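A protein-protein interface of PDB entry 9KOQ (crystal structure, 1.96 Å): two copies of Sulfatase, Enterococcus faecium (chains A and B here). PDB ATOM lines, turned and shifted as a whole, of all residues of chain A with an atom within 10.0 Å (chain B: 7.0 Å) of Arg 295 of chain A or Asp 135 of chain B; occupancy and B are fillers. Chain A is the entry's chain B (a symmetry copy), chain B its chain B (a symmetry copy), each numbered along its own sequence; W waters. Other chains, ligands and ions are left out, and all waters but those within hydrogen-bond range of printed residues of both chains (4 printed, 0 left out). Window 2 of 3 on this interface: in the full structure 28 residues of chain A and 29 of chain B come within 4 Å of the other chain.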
ATOM      1  N   ASN A   9     -29.186 -21.375  -4.044  1.00  0.00           N
ATOM      2  CA  ASN A   9     -28.685 -20.039  -3.757  1.00  0.00           C
ATOM      3  C   ASN A   9     -27.913 -19.505  -4.958  1.00  0.00           C
ATOM      4  O   ASN A   9     -27.449 -20.260  -5.817  1.00  0.00           O
ATOM      5  CB  ASN A   9     -27.777 -20.040  -2.527  1.00  0.00           C
ATOM      6  CG  ASN A   9     -28.383 -20.807  -1.365  1.00  0.00           C
ATOM      7  OD1 ASN A   9     -29.353 -20.356  -0.752  1.00  0.00           O
ATOM      8  ND2 ASN A   9     -27.792 -21.960  -1.037  1.00  0.00           N
ATOM      9  N   LEU A 197     -22.857 -14.714   5.347  1.00  0.00           N
ATOM     10  CA  LEU A 197     -23.181 -16.138   5.437  1.00  0.00           C
ATOM     11  C   LEU A 197     -23.401 -16.563   6.888  1.00  0.00           C
ATOM     12  O   LEU A 197     -24.341 -17.309   7.190  1.00  0.00           O
ATOM     13  CB  LEU A 197     -22.075 -16.984   4.802  1.00  0.00           C
ATOM     14  CG  LEU A 197     -21.895 -16.898   3.286  1.00  0.00           C
ATOM     15  CD1 LEU A 197     -20.710 -17.756   2.864  1.00  0.00           C
ATOM     16  CD2 LEU A 197     -23.186 -17.299   2.553  1.00  0.00           C
ATOM     17  N   ARG A 198     -22.544 -16.092   7.793  1.00  0.00           N
ATOM     18  CA  ARG A 198     -22.713 -16.365   9.219  1.00  0.00           C
ATOM     19  C   ARG A 198     -24.075 -15.911   9.731  1.00  0.00           C
ATOM     20  O   ARG A 198     -24.739 -16.628  10.489  1.00  0.00           O
ATOM     21  CB  ARG A 198     -21.614 -15.647   9.997  1.00  0.00           C
ATOM     22  CG  ARG A 198     -20.250 -16.284   9.876  1.00  0.00           C
ATOM     23  CD  ARG A 198     -19.260 -15.503  10.699  1.00  0.00           C
ATOM     24  NE  ARG A 198     -17.946 -16.123  10.680  1.00  0.00           N
ATOM     25  CZ  ARG A 198     -16.905 -15.682  11.374  1.00  0.00           C
ATOM     26  NH1 ARG A 198     -16.970 -14.559  12.077  1.00  0.00           N
ATOM     27  NH2 ARG A 198     -15.774 -16.384  11.364  1.00  0.00           N
ATOM     28  N   LYS A 200     -26.939 -14.806   8.075  1.00  0.00           N
ATOM     29  CA  LYS A 200     -28.132 -14.792   7.225  1.00  0.00           C
ATOM     30  C   LYS A 200     -29.290 -15.569   7.849  1.00  0.00           C
ATOM     31  O   LYS A 200     -29.113 -16.406   8.738  1.00  0.00           O
ATOM     32  CB  LYS A 200     -27.833 -15.391   5.854  1.00  0.00           C
ATOM     33  CG  LYS A 200     -27.522 -16.878   5.884  1.00  0.00           C
ATOM     34  CD  LYS A 200     -27.079 -17.355   4.496  1.00  0.00           C
ATOM     35  CE  LYS A 200     -26.484 -18.742   4.558  1.00  0.00           C
ATOM     36  NZ  LYS A 200     -27.513 -19.726   4.979  1.00  0.00           N
ATOM     37  N   PRO A 202     -31.555 -18.443   8.168  1.00  0.00           N
ATOM     38  CA  PRO A 202     -31.383 -19.835   7.736  1.00  0.00           C
ATOM     39  C   PRO A 202     -32.616 -20.455   7.101  1.00  0.00           C
ATOM     40  O   PRO A 202     -32.493 -21.548   6.541  1.00  0.00           O
ATOM     41  CB  PRO A 202     -31.021 -20.556   9.040  1.00  0.00           C
ATOM     42  CG  PRO A 202     -31.756 -19.791  10.085  1.00  0.00           C
ATOM     43  CD  PRO A 202     -31.734 -18.342   9.629  1.00  0.00           C
ATOM     44  N   PHE A 206     -30.502 -17.609  -0.402  1.00  0.00           N
ATOM     45  CA  PHE A 206     -29.926 -16.275  -0.531  1.00  0.00           C
ATOM     46  C   PHE A 206     -29.532 -15.960  -1.971  1.00  0.00           C
ATOM     47  O   PHE A 206     -29.144 -16.840  -2.745  1.00  0.00           O
ATOM     48  CB  PHE A 206     -28.712 -16.072   0.404  1.00  0.00           C
ATOM     49  CG  PHE A 206     -27.571 -16.998   0.147  1.00  0.00           C
ATOM     50  CD1 PHE A 206     -26.583 -16.674  -0.771  1.00  0.00           C
ATOM     51  CD2 PHE A 206     -27.460 -18.185   0.851  1.00  0.00           C
ATOM     52  CE1 PHE A 206     -25.513 -17.528  -0.995  1.00  0.00           C
ATOM     53  CE2 PHE A 206     -26.391 -19.041   0.634  1.00  0.00           C
ATOM     54  CZ  PHE A 206     -25.420 -18.713  -0.291  1.00  0.00           C
ATOM     55  N   PHE A 287     -13.568 -17.111  -0.413  1.00  0.00           N
ATOM     56  CA  PHE A 287     -15.019 -17.165  -0.303  1.00  0.00           C
ATOM     57  C   PHE A 287     -15.555 -18.546  -0.669  1.00  0.00           C
ATOM     58  O   PHE A 287     -16.517 -19.027  -0.060  1.00  0.00           O
ATOM     59  CB  PHE A 287     -15.668 -16.094  -1.192  1.00  0.00           C
ATOM     60  CG  PHE A 287     -17.161 -16.069  -1.081  1.00  0.00           C
ATOM     61  CD1 PHE A 287     -17.767 -15.449   0.006  1.00  0.00           C
ATOM     62  CD2 PHE A 287     -17.962 -16.698  -2.025  1.00  0.00           C
ATOM     63  CE1 PHE A 287     -19.157 -15.447   0.145  1.00  0.00           C
ATOM     64  CE2 PHE A 287     -19.333 -16.685  -1.898  1.00  0.00           C
ATOM     65  CZ  PHE A 287     -19.933 -16.059  -0.812  1.00  0.00           C
ATOM     66  N   LEU A 288     -14.949 -19.199  -1.665  1.00  0.00           N
ATOM     67  CA  LEU A 288     -15.355 -20.557  -2.006  1.00  0.00           C
ATOM     68  C   LEU A 288     -15.132 -21.509  -0.836  1.00  0.00           C
ATOM     69  O   LEU A 288     -15.988 -22.347  -0.540  1.00  0.00           O
ATOM     70  CB  LEU A 288     -14.593 -21.039  -3.239  1.00  0.00           C
ATOM     71  CG  LEU A 288     -14.815 -20.324  -4.580  1.00  0.00           C
ATOM     72  CD1 LEU A 288     -14.028 -21.043  -5.667  1.00  0.00           C
ATOM     73  CD2 LEU A 288     -16.297 -20.274  -4.925  1.00  0.00           C
ATOM     74  N   MET A 289     -13.987 -21.394  -0.158  1.00  0.00           N
ATOM     75  CA  MET A 289     -13.724 -22.237   1.004  1.00  0.00           C
ATOM     76  C   MET A 289     -14.781 -22.010   2.080  1.00  0.00           C
ATOM     77  O   MET A 289     -15.270 -22.963   2.696  1.00  0.00           O
ATOM     78  CB  MET A 289     -12.329 -21.926   1.529  1.00  0.00           C
ATOM     79  CG  MET A 289     -11.246 -22.534   0.647  1.00  0.00           C
ATOM     80  SD  MET A 289      -9.589 -22.504   1.368  1.00  0.00           S
ATOM     81  CE  MET A 289      -9.189 -20.763   1.249  1.00  0.00           C
ATOM     82  N   ALA A 290     -15.176 -20.751   2.292  1.00  0.00           N
ATOM     83  CA  ALA A 290     -16.198 -20.458   3.294  1.00  0.00           C
ATOM     84  C   ALA A 290     -17.551 -21.022   2.893  1.00  0.00           C
ATOM     85  O   ALA A 290     -18.302 -21.497   3.751  1.00  0.00           O
ATOM     86  CB  ALA A 290     -16.313 -18.950   3.532  1.00  0.00           C
ATOM     87  N   LEU A 291     -17.901 -20.951   1.605  1.00  0.00           N
ATOM     88  CA  LEU A 291     -19.164 -21.541   1.168  1.00  0.00           C
ATOM     89  C   LEU A 291     -19.240 -23.008   1.565  1.00  0.00           C
ATOM     90  O   LEU A 291     -20.301 -23.509   1.957  1.00  0.00           O
ATOM     91  CB  LEU A 291     -19.313 -21.394  -0.345  1.00  0.00           C
ATOM     92  CG  LEU A 291     -19.986 -20.171  -0.950  1.00  0.00           C
ATOM     93  CD1 LEU A 291     -20.027 -20.357  -2.481  1.00  0.00           C
ATOM     94  CD2 LEU A 291     -21.397 -19.956  -0.387  1.00  0.00           C
ATOM     95  N   LYS A 292     -18.112 -23.709   1.475  1.00  0.00           N
ATOM     96  CA  LYS A 292     -18.079 -25.123   1.827  1.00  0.00           C
ATOM     97  C   LYS A 292     -18.236 -25.329   3.334  1.00  0.00           C
ATOM     98  O   LYS A 292     -18.902 -26.276   3.773  1.00  0.00           O
ATOM     99  CB  LYS A 292     -16.774 -25.740   1.320  1.00  0.00           C
ATOM    100  CG  LYS A 292     -16.674 -27.239   1.565  1.00  0.00           C
ATOM    101  CD  LYS A 292     -15.336 -27.787   1.095  1.00  0.00           C
ATOM    102  CE  LYS A 292     -15.488 -29.171   0.482  1.00  0.00           C
ATOM    103  NZ  LYS A 292     -14.968 -29.207  -0.918  1.00  0.00           N
ATOM    104  N   GLU A 293     -17.640 -24.447   4.143  1.00  0.00           N
ATOM    105  CA  GLU A 293     -17.833 -24.518   5.591  1.00  0.00           C
ATOM    106  C   GLU A 293     -19.299 -24.361   5.969  1.00  0.00           C
ATOM    107  O   GLU A 293     -19.739 -24.906   6.992  1.00  0.00           O
ATOM    108  CB  GLU A 293     -16.974 -23.446   6.268  1.00  0.00           C
ATOM    109  CG  GLU A 293     -15.468 -23.613   5.953  1.00  0.00           C
ATOM    110  CD  GLU A 293     -14.574 -22.574   6.641  1.00  0.00           C
ATOM    111  OE1 GLU A 293     -13.336 -22.772   6.664  1.00  0.00           O
ATOM    112  OE2 GLU A 293     -15.085 -21.517   7.064  1.00  0.00           O
ATOM    113  N   PHE A 294     -20.067 -23.617   5.175  1.00  0.00           N
ATOM    114  CA  PHE A 294     -21.493 -23.463   5.423  1.00  0.00           C
ATOM    115  C   PHE A 294     -22.330 -24.519   4.717  1.00  0.00           C
ATOM    116  O   PHE A 294     -23.563 -24.428   4.744  1.00  0.00           O
ATOM    117  CB  PHE A 294     -21.954 -22.072   5.000  1.00  0.00           C
ATOM    118  CG  PHE A 294     -21.486 -20.983   5.917  1.00  0.00           C
ATOM    119  CD1 PHE A 294     -22.167 -20.715   7.095  1.00  0.00           C
ATOM    120  CD2 PHE A 294     -20.386 -20.206   5.585  1.00  0.00           C
ATOM    121  CE1 PHE A 294     -21.737 -19.711   7.939  1.00  0.00           C
ATOM    122  CE2 PHE A 294     -19.958 -19.196   6.424  1.00  0.00           C
ATOM    123  CZ  PHE A 294     -20.639 -18.949   7.599  1.00  0.00           C
ATOM    124  N   ARG A 295     -21.685 -25.517   4.109  1.00  0.00           N
ATOM    125  CA  ARG A 295     -22.356 -26.563   3.326  1.00  0.00           C
ATOM    126  C   ARG A 295     -23.207 -25.964   2.210  1.00  0.00           C
ATOM    127  O   ARG A 295     -24.309 -26.437   1.922  1.00  0.00           O
ATOM    128  CB  ARG A 295     -23.205 -27.477   4.219  1.00  0.00           C
ATOM    129  CG  ARG A 295     -22.397 -28.288   5.223  1.00  0.00           C
ATOM    130  CD  ARG A 295     -23.250 -29.405   5.828  1.00  0.00           C
ATOM    131  NE  ARG A 295     -22.626 -29.996   7.007  1.00  0.00           N
ATOM    132  CZ  ARG A 295     -21.696 -30.939   6.978  1.00  0.00           C
ATOM    133  NH1 ARG A 295     -21.258 -31.443   5.836  1.00  0.00           N
ATOM    134  NH2 ARG A 295     -21.205 -31.397   8.125  1.00  0.00           N
ATOM    135  N   HIS A 296     -22.703 -24.901   1.580  1.00  0.00           N
ATOM    136  CA  HIS A 296     -23.400 -24.292   0.459  1.00  0.00           C
ATOM    137  C   HIS A 296     -22.628 -24.426  -0.841  1.00  0.00           C
ATOM    138  O   HIS A 296     -22.980 -23.768  -1.823  1.00  0.00           O
ATOM    139  CB  HIS A 296     -23.687 -22.820   0.738  1.00  0.00           C
ATOM    140  CG  HIS A 296     -24.801 -22.624   1.707  1.00  0.00           C
ATOM    141  ND1 HIS A 296     -25.964 -23.359   1.653  1.00  0.00           N
ATOM    142  CD2 HIS A 296     -24.920 -21.800   2.773  1.00  0.00           C
ATOM    143  CE1 HIS A 296     -26.756 -22.989   2.642  1.00  0.00           C
ATOM    144  NE2 HIS A 296     -26.146 -22.044   3.334  1.00  0.00           N
ATOM    145  N   ASP A 297     -21.596 -25.268  -0.877  1.00  0.00           N
ATOM    146  CA  ASP A 297     -20.785 -25.390  -2.080  1.00  0.00           C
ATOM    147  C   ASP A 297     -21.498 -26.140  -3.198  1.00  0.00           C
ATOM    148  O   ASP A 297     -21.128 -25.973  -4.367  1.00  0.00           O
ATOM    149  CB  ASP A 297     -19.458 -26.080  -1.751  1.00  0.00           C
ATOM    150  CG  ASP A 297     -19.650 -27.398  -1.025  1.00  0.00           C
ATOM    151  OD1 ASP A 297     -20.476 -27.465  -0.085  1.00  0.00           O
ATOM    152  OD2 ASP A 297     -18.966 -28.370  -1.402  1.00  0.00           O
ATOM    153  N   LYS A 298     -22.525 -26.931  -2.878  1.00  0.00           N
ATOM    154  CA  LYS A 298     -23.196 -27.765  -3.866  1.00  0.00           C
ATOM    155  C   LYS A 298     -24.626 -27.318  -4.158  1.00  0.00           C
ATOM    156  O   LYS A 298     -25.276 -27.905  -5.032  1.00  0.00           O
ATOM    157  CB  LYS A 298     -23.218 -29.226  -3.392  1.00  0.00           C
ATOM    158  CG  LYS A 298     -21.862 -29.899  -3.263  1.00  0.00           C
ATOM    159  CD  LYS A 298     -20.976 -29.740  -4.475  1.00  0.00           C
ATOM    160  CE  LYS A 298     -19.753 -30.654  -4.342  1.00  0.00           C
ATOM    161  NZ  LYS A 298     -18.678 -30.341  -5.335  1.00  0.00           N
ATOM    162  N   ASP A 299     -25.156 -26.325  -3.438  1.00  0.00           N
ATOM    163  CA  ASP A 299     -26.512 -25.848  -3.692  1.00  0.00           C
ATOM    164  C   ASP A 299     -26.529 -24.377  -4.107  1.00  0.00           C
ATOM    165  O   ASP A 299     -27.553 -23.698  -3.967  1.00  0.00           O
ATOM    166  CB  ASP A 299     -27.411 -26.098  -2.474  1.00  0.00           C
ATOM    167  CG  ASP A 299     -26.990 -25.293  -1.235  1.00  0.00           C
ATOM    168  OD1 ASP A 299     -25.997 -24.535  -1.303  1.00  0.00           O
ATOM    169  OD2 ASP A 299     -27.668 -25.421  -0.187  1.00  0.00           O
ATOM    170  N   THR A 300     -25.413 -23.876  -4.628  1.00  0.00           N
ATOM    171  CA  THR A 300     -25.257 -22.471  -4.970  1.00  0.00           C
ATOM    172  C   THR A 300     -24.748 -22.364  -6.397  1.00  0.00           C
ATOM    173  O   THR A 300     -23.859 -23.120  -6.801  1.00  0.00           O
ATOM    174  CB  THR A 300     -24.261 -21.786  -4.003  1.00  0.00           C
ATOM    175  OG1 THR A 300     -24.828 -21.760  -2.696  1.00  0.00           O
ATOM    176  CG2 THR A 300     -23.968 -20.369  -4.434  1.00  0.00           C
ATOM    177  N   GLY A 338     -22.247 -27.881  -8.029  1.00  0.00           N
ATOM    178  CA  GLY A 338     -23.251 -28.858  -7.656  1.00  0.00           C
ATOM    179  C   GLY A 338     -23.975 -29.484  -8.822  1.00  0.00           C
ATOM    180  O   GLY A 338     -24.866 -30.311  -8.619  1.00  0.00           O
ATOM    181  N   HIS B 129     -11.591 -30.177   7.346  1.00  0.00           N
ATOM    182  CA  HIS B 129     -12.981 -29.948   6.955  1.00  0.00           C
ATOM    183  C   HIS B 129     -13.959 -30.458   8.009  1.00  0.00           C
ATOM    184  O   HIS B 129     -15.002 -29.835   8.242  1.00  0.00           O
ATOM    185  CB  HIS B 129     -13.266 -30.588   5.592  1.00  0.00           C
ATOM    186  CG  HIS B 129     -12.491 -29.976   4.461  1.00  0.00           C
ATOM    187  ND1 HIS B 129     -13.010 -28.980   3.657  1.00  0.00           N
ATOM    188  CD2 HIS B 129     -11.242 -30.221   3.992  1.00  0.00           C
ATOM    189  CE1 HIS B 129     -12.111 -28.632   2.751  1.00  0.00           C
ATOM    190  NE2 HIS B 129     -11.031 -29.371   2.932  1.00  0.00           N
ATOM    191  N   VAL B 130     -13.634 -31.568   8.683  1.00  0.00           N
ATOM    192  CA  VAL B 130     -14.573 -32.112   9.659  1.00  0.00           C
ATOM    193  C   VAL B 130     -14.636 -31.291  10.942  1.00  0.00           C
ATOM    194  O   VAL B 130     -15.543 -31.517  11.759  1.00  0.00           O
ATOM    195  CB  VAL B 130     -14.240 -33.578  10.005  1.00  0.00           C
ATOM    196  CG1 VAL B 130     -14.586 -34.489   8.814  1.00  0.00           C
ATOM    197  CG2 VAL B 130     -12.786 -33.713  10.461  1.00  0.00           C
ATOM    198  N   ARG B 132     -14.455 -27.785  10.606  1.00  0.00           N
ATOM    199  CA  ARG B 132     -14.768 -26.443  10.108  1.00  0.00           C
ATOM    200  C   ARG B 132     -16.122 -26.460   9.399  1.00  0.00           C
ATOM    201  O   ARG B 132     -16.254 -26.092   8.232  1.00  0.00           O
ATOM    202  CB  ARG B 132     -13.637 -25.924   9.218  1.00  0.00           C
ATOM    203  CG  ARG B 132     -12.297 -25.916   9.957  1.00  0.00           C
ATOM    204  CD  ARG B 132     -11.303 -24.888   9.464  1.00  0.00           C
ATOM    205  NE  ARG B 132     -11.877 -23.645   8.948  1.00  0.00           N
ATOM    206  CZ  ARG B 132     -11.583 -22.436   9.414  1.00  0.00           C
ATOM    207  NH1 ARG B 132     -10.802 -22.274  10.477  1.00  0.00           N
ATOM    208  NH2 ARG B 132     -12.063 -21.364   8.787  1.00  0.00           N
ATOM    209  N   LYS B 133     -17.149 -26.887  10.134  1.00  0.00           N
ATOM    210  CA  LYS B 133     -18.526 -26.879   9.648  1.00  0.00           C
ATOM    211  C   LYS B 133     -19.375 -26.073  10.626  1.00  0.00           C
ATOM    212  O   LYS B 133     -19.471 -26.424  11.811  1.00  0.00           O
ATOM    213  CB  LYS B 133     -19.064 -28.309   9.488  1.00  0.00           C
ATOM    214  CG  LYS B 133     -18.380 -29.101   8.368  1.00  0.00           C
ATOM    215  CD  LYS B 133     -18.714 -28.479   7.003  1.00  0.00           C
ATOM    216  CE  LYS B 133     -18.374 -29.408   5.844  1.00  0.00           C
ATOM    217  NZ  LYS B 133     -16.891 -29.499   5.632  1.00  0.00           N
ATOM    218  N   TYR B 134     -19.989 -24.996  10.121  1.00  0.00           N
ATOM    219  CA  TYR B 134     -20.805 -24.107  10.940  1.00  0.00           C
ATOM    220  C   TYR B 134     -21.990 -24.811  11.588  1.00  0.00           C
ATOM    221  O   TYR B 134     -22.504 -24.320  12.599  1.00  0.00           O
ATOM    222  CB  TYR B 134     -21.276 -22.931  10.075  1.00  0.00           C
ATOM    223  CG  TYR B 134     -20.241 -21.822   9.971  1.00  0.00           C
ATOM    224  CD1 TYR B 134     -20.187 -20.790  10.909  1.00  0.00           C
ATOM    225  CD2 TYR B 134     -19.262 -21.854   8.978  1.00  0.00           C
ATOM    226  CE1 TYR B 134     -19.226 -19.777  10.815  1.00  0.00           C
ATOM    227  CE2 TYR B 134     -18.288 -20.852   8.879  1.00  0.00           C
ATOM    228  CZ  TYR B 134     -18.271 -19.820   9.803  1.00  0.00           C
ATOM    229  OH  TYR B 134     -17.304 -18.826   9.697  1.00  0.00           O
ATOM    230  N   ASP B 135     -22.432 -25.955  11.060  1.00  0.00           N
ATOM    231  CA  ASP B 135     -23.559 -26.641  11.680  1.00  0.00           C
ATOM    232  C   ASP B 135     -23.158 -27.748  12.653  1.00  0.00           C
ATOM    233  O   ASP B 135     -24.044 -28.352  13.259  1.00  0.00           O
ATOM    234  CB  ASP B 135     -24.527 -27.197  10.618  1.00  0.00           C
ATOM    235  CG  ASP B 135     -23.899 -28.234   9.693  1.00  0.00           C
ATOM    236  OD1 ASP B 135     -22.766 -28.705   9.929  1.00  0.00           O
ATOM    237  OD2 ASP B 135     -24.590 -28.605   8.715  1.00  0.00           O
ATOM    238  N   LYS B 136     -21.862 -28.022  12.838  1.00  0.00           N
ATOM    239  CA  LYS B 136     -21.441 -29.032  13.804  1.00  0.00           C
ATOM    240  C   LYS B 136     -21.147 -28.391  15.173  1.00  0.00           C
ATOM    241  O   LYS B 136     -21.165 -27.170  15.329  1.00  0.00           O
ATOM    242  CB  LYS B 136     -20.235 -29.808  13.260  1.00  0.00           C
ATOM    243  CG  LYS B 136     -20.588 -30.624  11.988  1.00  0.00           C
ATOM    244  CD  LYS B 136     -19.375 -31.330  11.360  1.00  0.00           C
ATOM    245  CE  LYS B 136     -18.829 -32.430  12.267  1.00  0.00           C
ATOM    246  NZ  LYS B 136     -17.791 -33.258  11.579  1.00  0.00           N
ATOM    247  N   SER B 137     -20.884 -29.241  16.173  1.00  0.00           N
ATOM    248  CA  SER B 137     -20.820 -28.804  17.574  1.00  0.00           C
ATOM    249  C   SER B 137     -19.844 -27.656  17.795  1.00  0.00           C
ATOM    250  O   SER B 137     -18.671 -27.739  17.425  1.00  0.00           O
ATOM    251  CB  SER B 137     -20.426 -29.973  18.483  1.00  0.00           C
ATOM    252  OG  SER B 137     -21.509 -30.865  18.644  1.00  0.00           O
ATOM    253  N   TYR B 138     -20.339 -26.603  18.451  1.00  0.00           N
ATOM    254  CA  TYR B 138     -19.538 -25.407  18.711  1.00  0.00           C
ATOM    255  C   TYR B 138     -18.201 -25.749  19.357  1.00  0.00           C
ATOM    256  O   TYR B 138     -17.139 -25.324  18.883  1.00  0.00           O
ATOM    257  CB  TYR B 138     -20.358 -24.466  19.597  1.00  0.00           C
ATOM    258  CG  TYR B 138     -19.660 -23.266  20.191  1.00  0.00           C
ATOM    259  CD1 TYR B 138     -19.027 -23.337  21.433  1.00  0.00           C
ATOM    260  CD2 TYR B 138     -19.682 -22.028  19.528  1.00  0.00           C
ATOM    261  CE1 TYR B 138     -18.412 -22.221  21.994  1.00  0.00           C
ATOM    262  CE2 TYR B 138     -19.070 -20.897  20.092  1.00  0.00           C
ATOM    263  CZ  TYR B 138     -18.445 -21.003  21.326  1.00  0.00           C
ATOM    264  OH  TYR B 138     -17.845 -19.896  21.897  1.00  0.00           O
ATOM    265  N   GLN B 141     -15.473 -27.129  16.895  1.00  0.00           N
ATOM    266  CA  GLN B 141     -15.293 -26.525  15.579  1.00  0.00           C
ATOM    267  C   GLN B 141     -14.386 -25.301  15.660  1.00  0.00           C
ATOM    268  O   GLN B 141     -14.292 -24.630  16.692  1.00  0.00           O
ATOM    269  CB  GLN B 141     -16.639 -26.097  14.934  1.00  0.00           C
ATOM    270  CG  GLN B 141     -17.663 -27.187  14.542  1.00  0.00           C
ATOM    271  CD  GLN B 141     -17.089 -28.355  13.759  1.00  0.00           C
ATOM    272  OE1 GLN B 141     -16.986 -28.314  12.527  1.00  0.00           O
ATOM    273  NE2 GLN B 141     -16.802 -29.442  14.461  1.00  0.00           N
ATOM    274  N   PHE B 142     -13.735 -25.008  14.529  1.00  0.00           N
ATOM    275  CA  PHE B 142     -13.003 -23.760  14.315  1.00  0.00           C
ATOM    276  C   PHE B 142     -12.041 -23.439  15.455  1.00  0.00           C
ATOM    277  O   PHE B 142     -11.151 -24.245  15.741  1.00  0.00           O
ATOM    278  CB  PHE B 142     -13.986 -22.614  14.060  1.00  0.00           C
ATOM    279  CG  PHE B 142     -14.793 -22.798  12.779  1.00  0.00           C
ATOM    280  CD1 PHE B 142     -14.280 -22.375  11.558  1.00  0.00           C
ATOM    281  CD2 PHE B 142     -16.048 -23.401  12.802  1.00  0.00           C
ATOM    282  CE1 PHE B 142     -15.012 -22.557  10.365  1.00  0.00           C
ATOM    283  CE2 PHE B 142     -16.788 -23.582  11.619  1.00  0.00           C
ATOM    284  CZ  PHE B 142     -16.266 -23.164  10.403  1.00  0.00           C
HETATM  285  O   HOH W   1     -15.493 -18.976   7.688  1.00  0.00           O
HETATM  286  O   HOH W   2     -22.069 -26.070   7.974  1.00  0.00           O
HETATM  287  O   HOH W   3     -18.604 -33.393   8.422  1.00  0.00           O
HETATM  288  O   HOH W   4     -15.905 -18.906  12.198  1.00  0.00           O
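No position is printed for both chains.
Printed residues of chain A that touch a printed residue of chain B: Arg 198, Lys 292, Glu 293, Phe 294 and Arg 295.
Hydrophobic or aromatic side chains of chain A that line the printed part of chain B: Phe 294.
Along chain A the printed residues that touch a printed residue of chain B span positions 198 to 295.
Hydrophobic or aromatic side chains of chain B that line the printed part of chain A: His 129, Tyr 134 and Phe 142.
Among the printed residues, 11 pairs touch across the chains.
NZ of Lys 133 of chain B sits at hydrogen-bond distance from O of His 129 of chain B.
O of Val 130 of chain B is in hydrogen-bond range of NZ of Lys 136 of chain B (2.8 Å).
The backbone NH (N) of Arg 132 of chain B sits at hydrogen-bond distance from the side-chain amide oxygen (OE1) of Gln 141 of chain B (3.2 Å).
The side-chain amide oxygen of Gln 141 of chain B is in hydrogen-bond range of the backbone NH of Lys 133 of chain B, 2.8 Å away.
Arg 295 of chain A touches just these residues of chain B: Lys 133 (3.5 Å), Asp 135 (3.0 Å) and Lys 136 (3.7 Å).
Of the printed residues of chain A, Asp 135 of chain B touches Arg 295.
Printed residues of chain A within 4 Å of Lys 136 of chain B: Arg 295.
Of the printed residues of chain B, Lys 292 of chain A touches His 129 and Lys 133.
Printed residues of chain A within 4 Å of Phe 142 of chain B: Glu 293.
Printed residues of chain A within 4 Å of Tyr 134 of chain B: Arg 198 (2.9 Å), Glu 293 (3.1 Å) and Phe 294 (3.3 Å).
Asn 9 of chain A touches none of the printed residues of chain B.
Phe 206 of chain A touches none of the printed residues of chain B.
The nearest residue of chain A that does not touch Asp 135 of chain B is Glu 293 of chain A (5.0 Å).
Water W1 bridges the side-chain carboxylate of Glu 293 of chain A (2.6 Å) and the side-chain hydroxyl of Tyr 134 of chain B (2.7 Å).
Water W4 bridges the guanidinium group of Arg 198 of chain A and the side-chain hydroxyl of Tyr 134 of chain B.
Water W2 lies within hydrogen-bond range of the backbone carbonyl oxygen of Glu 293 of chain A (2.8 Å), the backbone NH of Asp 135 of chain B (3.1 Å) and the backbone NH of Tyr 134 of chain B (3.2 Å).
Water W3 lies within hydrogen-bond range of the side-chain amino group (NZ) of Lys 136 of chain B (3.3 Å) and the guanidinium group (NH2) of Arg 295 of chain A (3.3 Å).
Among the printed residues, pairs that only touch across the chains: Phe 294 of chain A with Tyr 134 of chain B (3.3 Å), Glu 293 of chain A with Phe 142 of chain B (3.5 Å), Glu 293 of chain A with Lys 133 of chain B (3.5 Å), Arg 295 of chain A with Lys 133 of chain B (3.5 Å), Lys 292 of chain A with His 129 of chain B (3.7 Å), Arg 295 of chain A with Lys 136 of chain B (3.7 Å) and Lys 292 of chain A with Lys 133 of chain B (3.8 Å).
OE1 of Glu 293 of chain A lies within salt-bridge range of NE of Arg 132 of chain B, 2.8 Å away.
The side-chain hydroxyl (OH) of Tyr 134 of chain B lies within hydrogen-bond range of the guanidinium group (NE) of Arg 198 of chain A (2.9 Å).
N of Tyr 134 of chain B sits at hydrogen-bond distance from O of Glu 293 of chain A (3.1 Å).
OD2 of Asp 135 of chain B is in salt-bridge range of NE of Arg 295 of chain A, at 3.0 Å.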
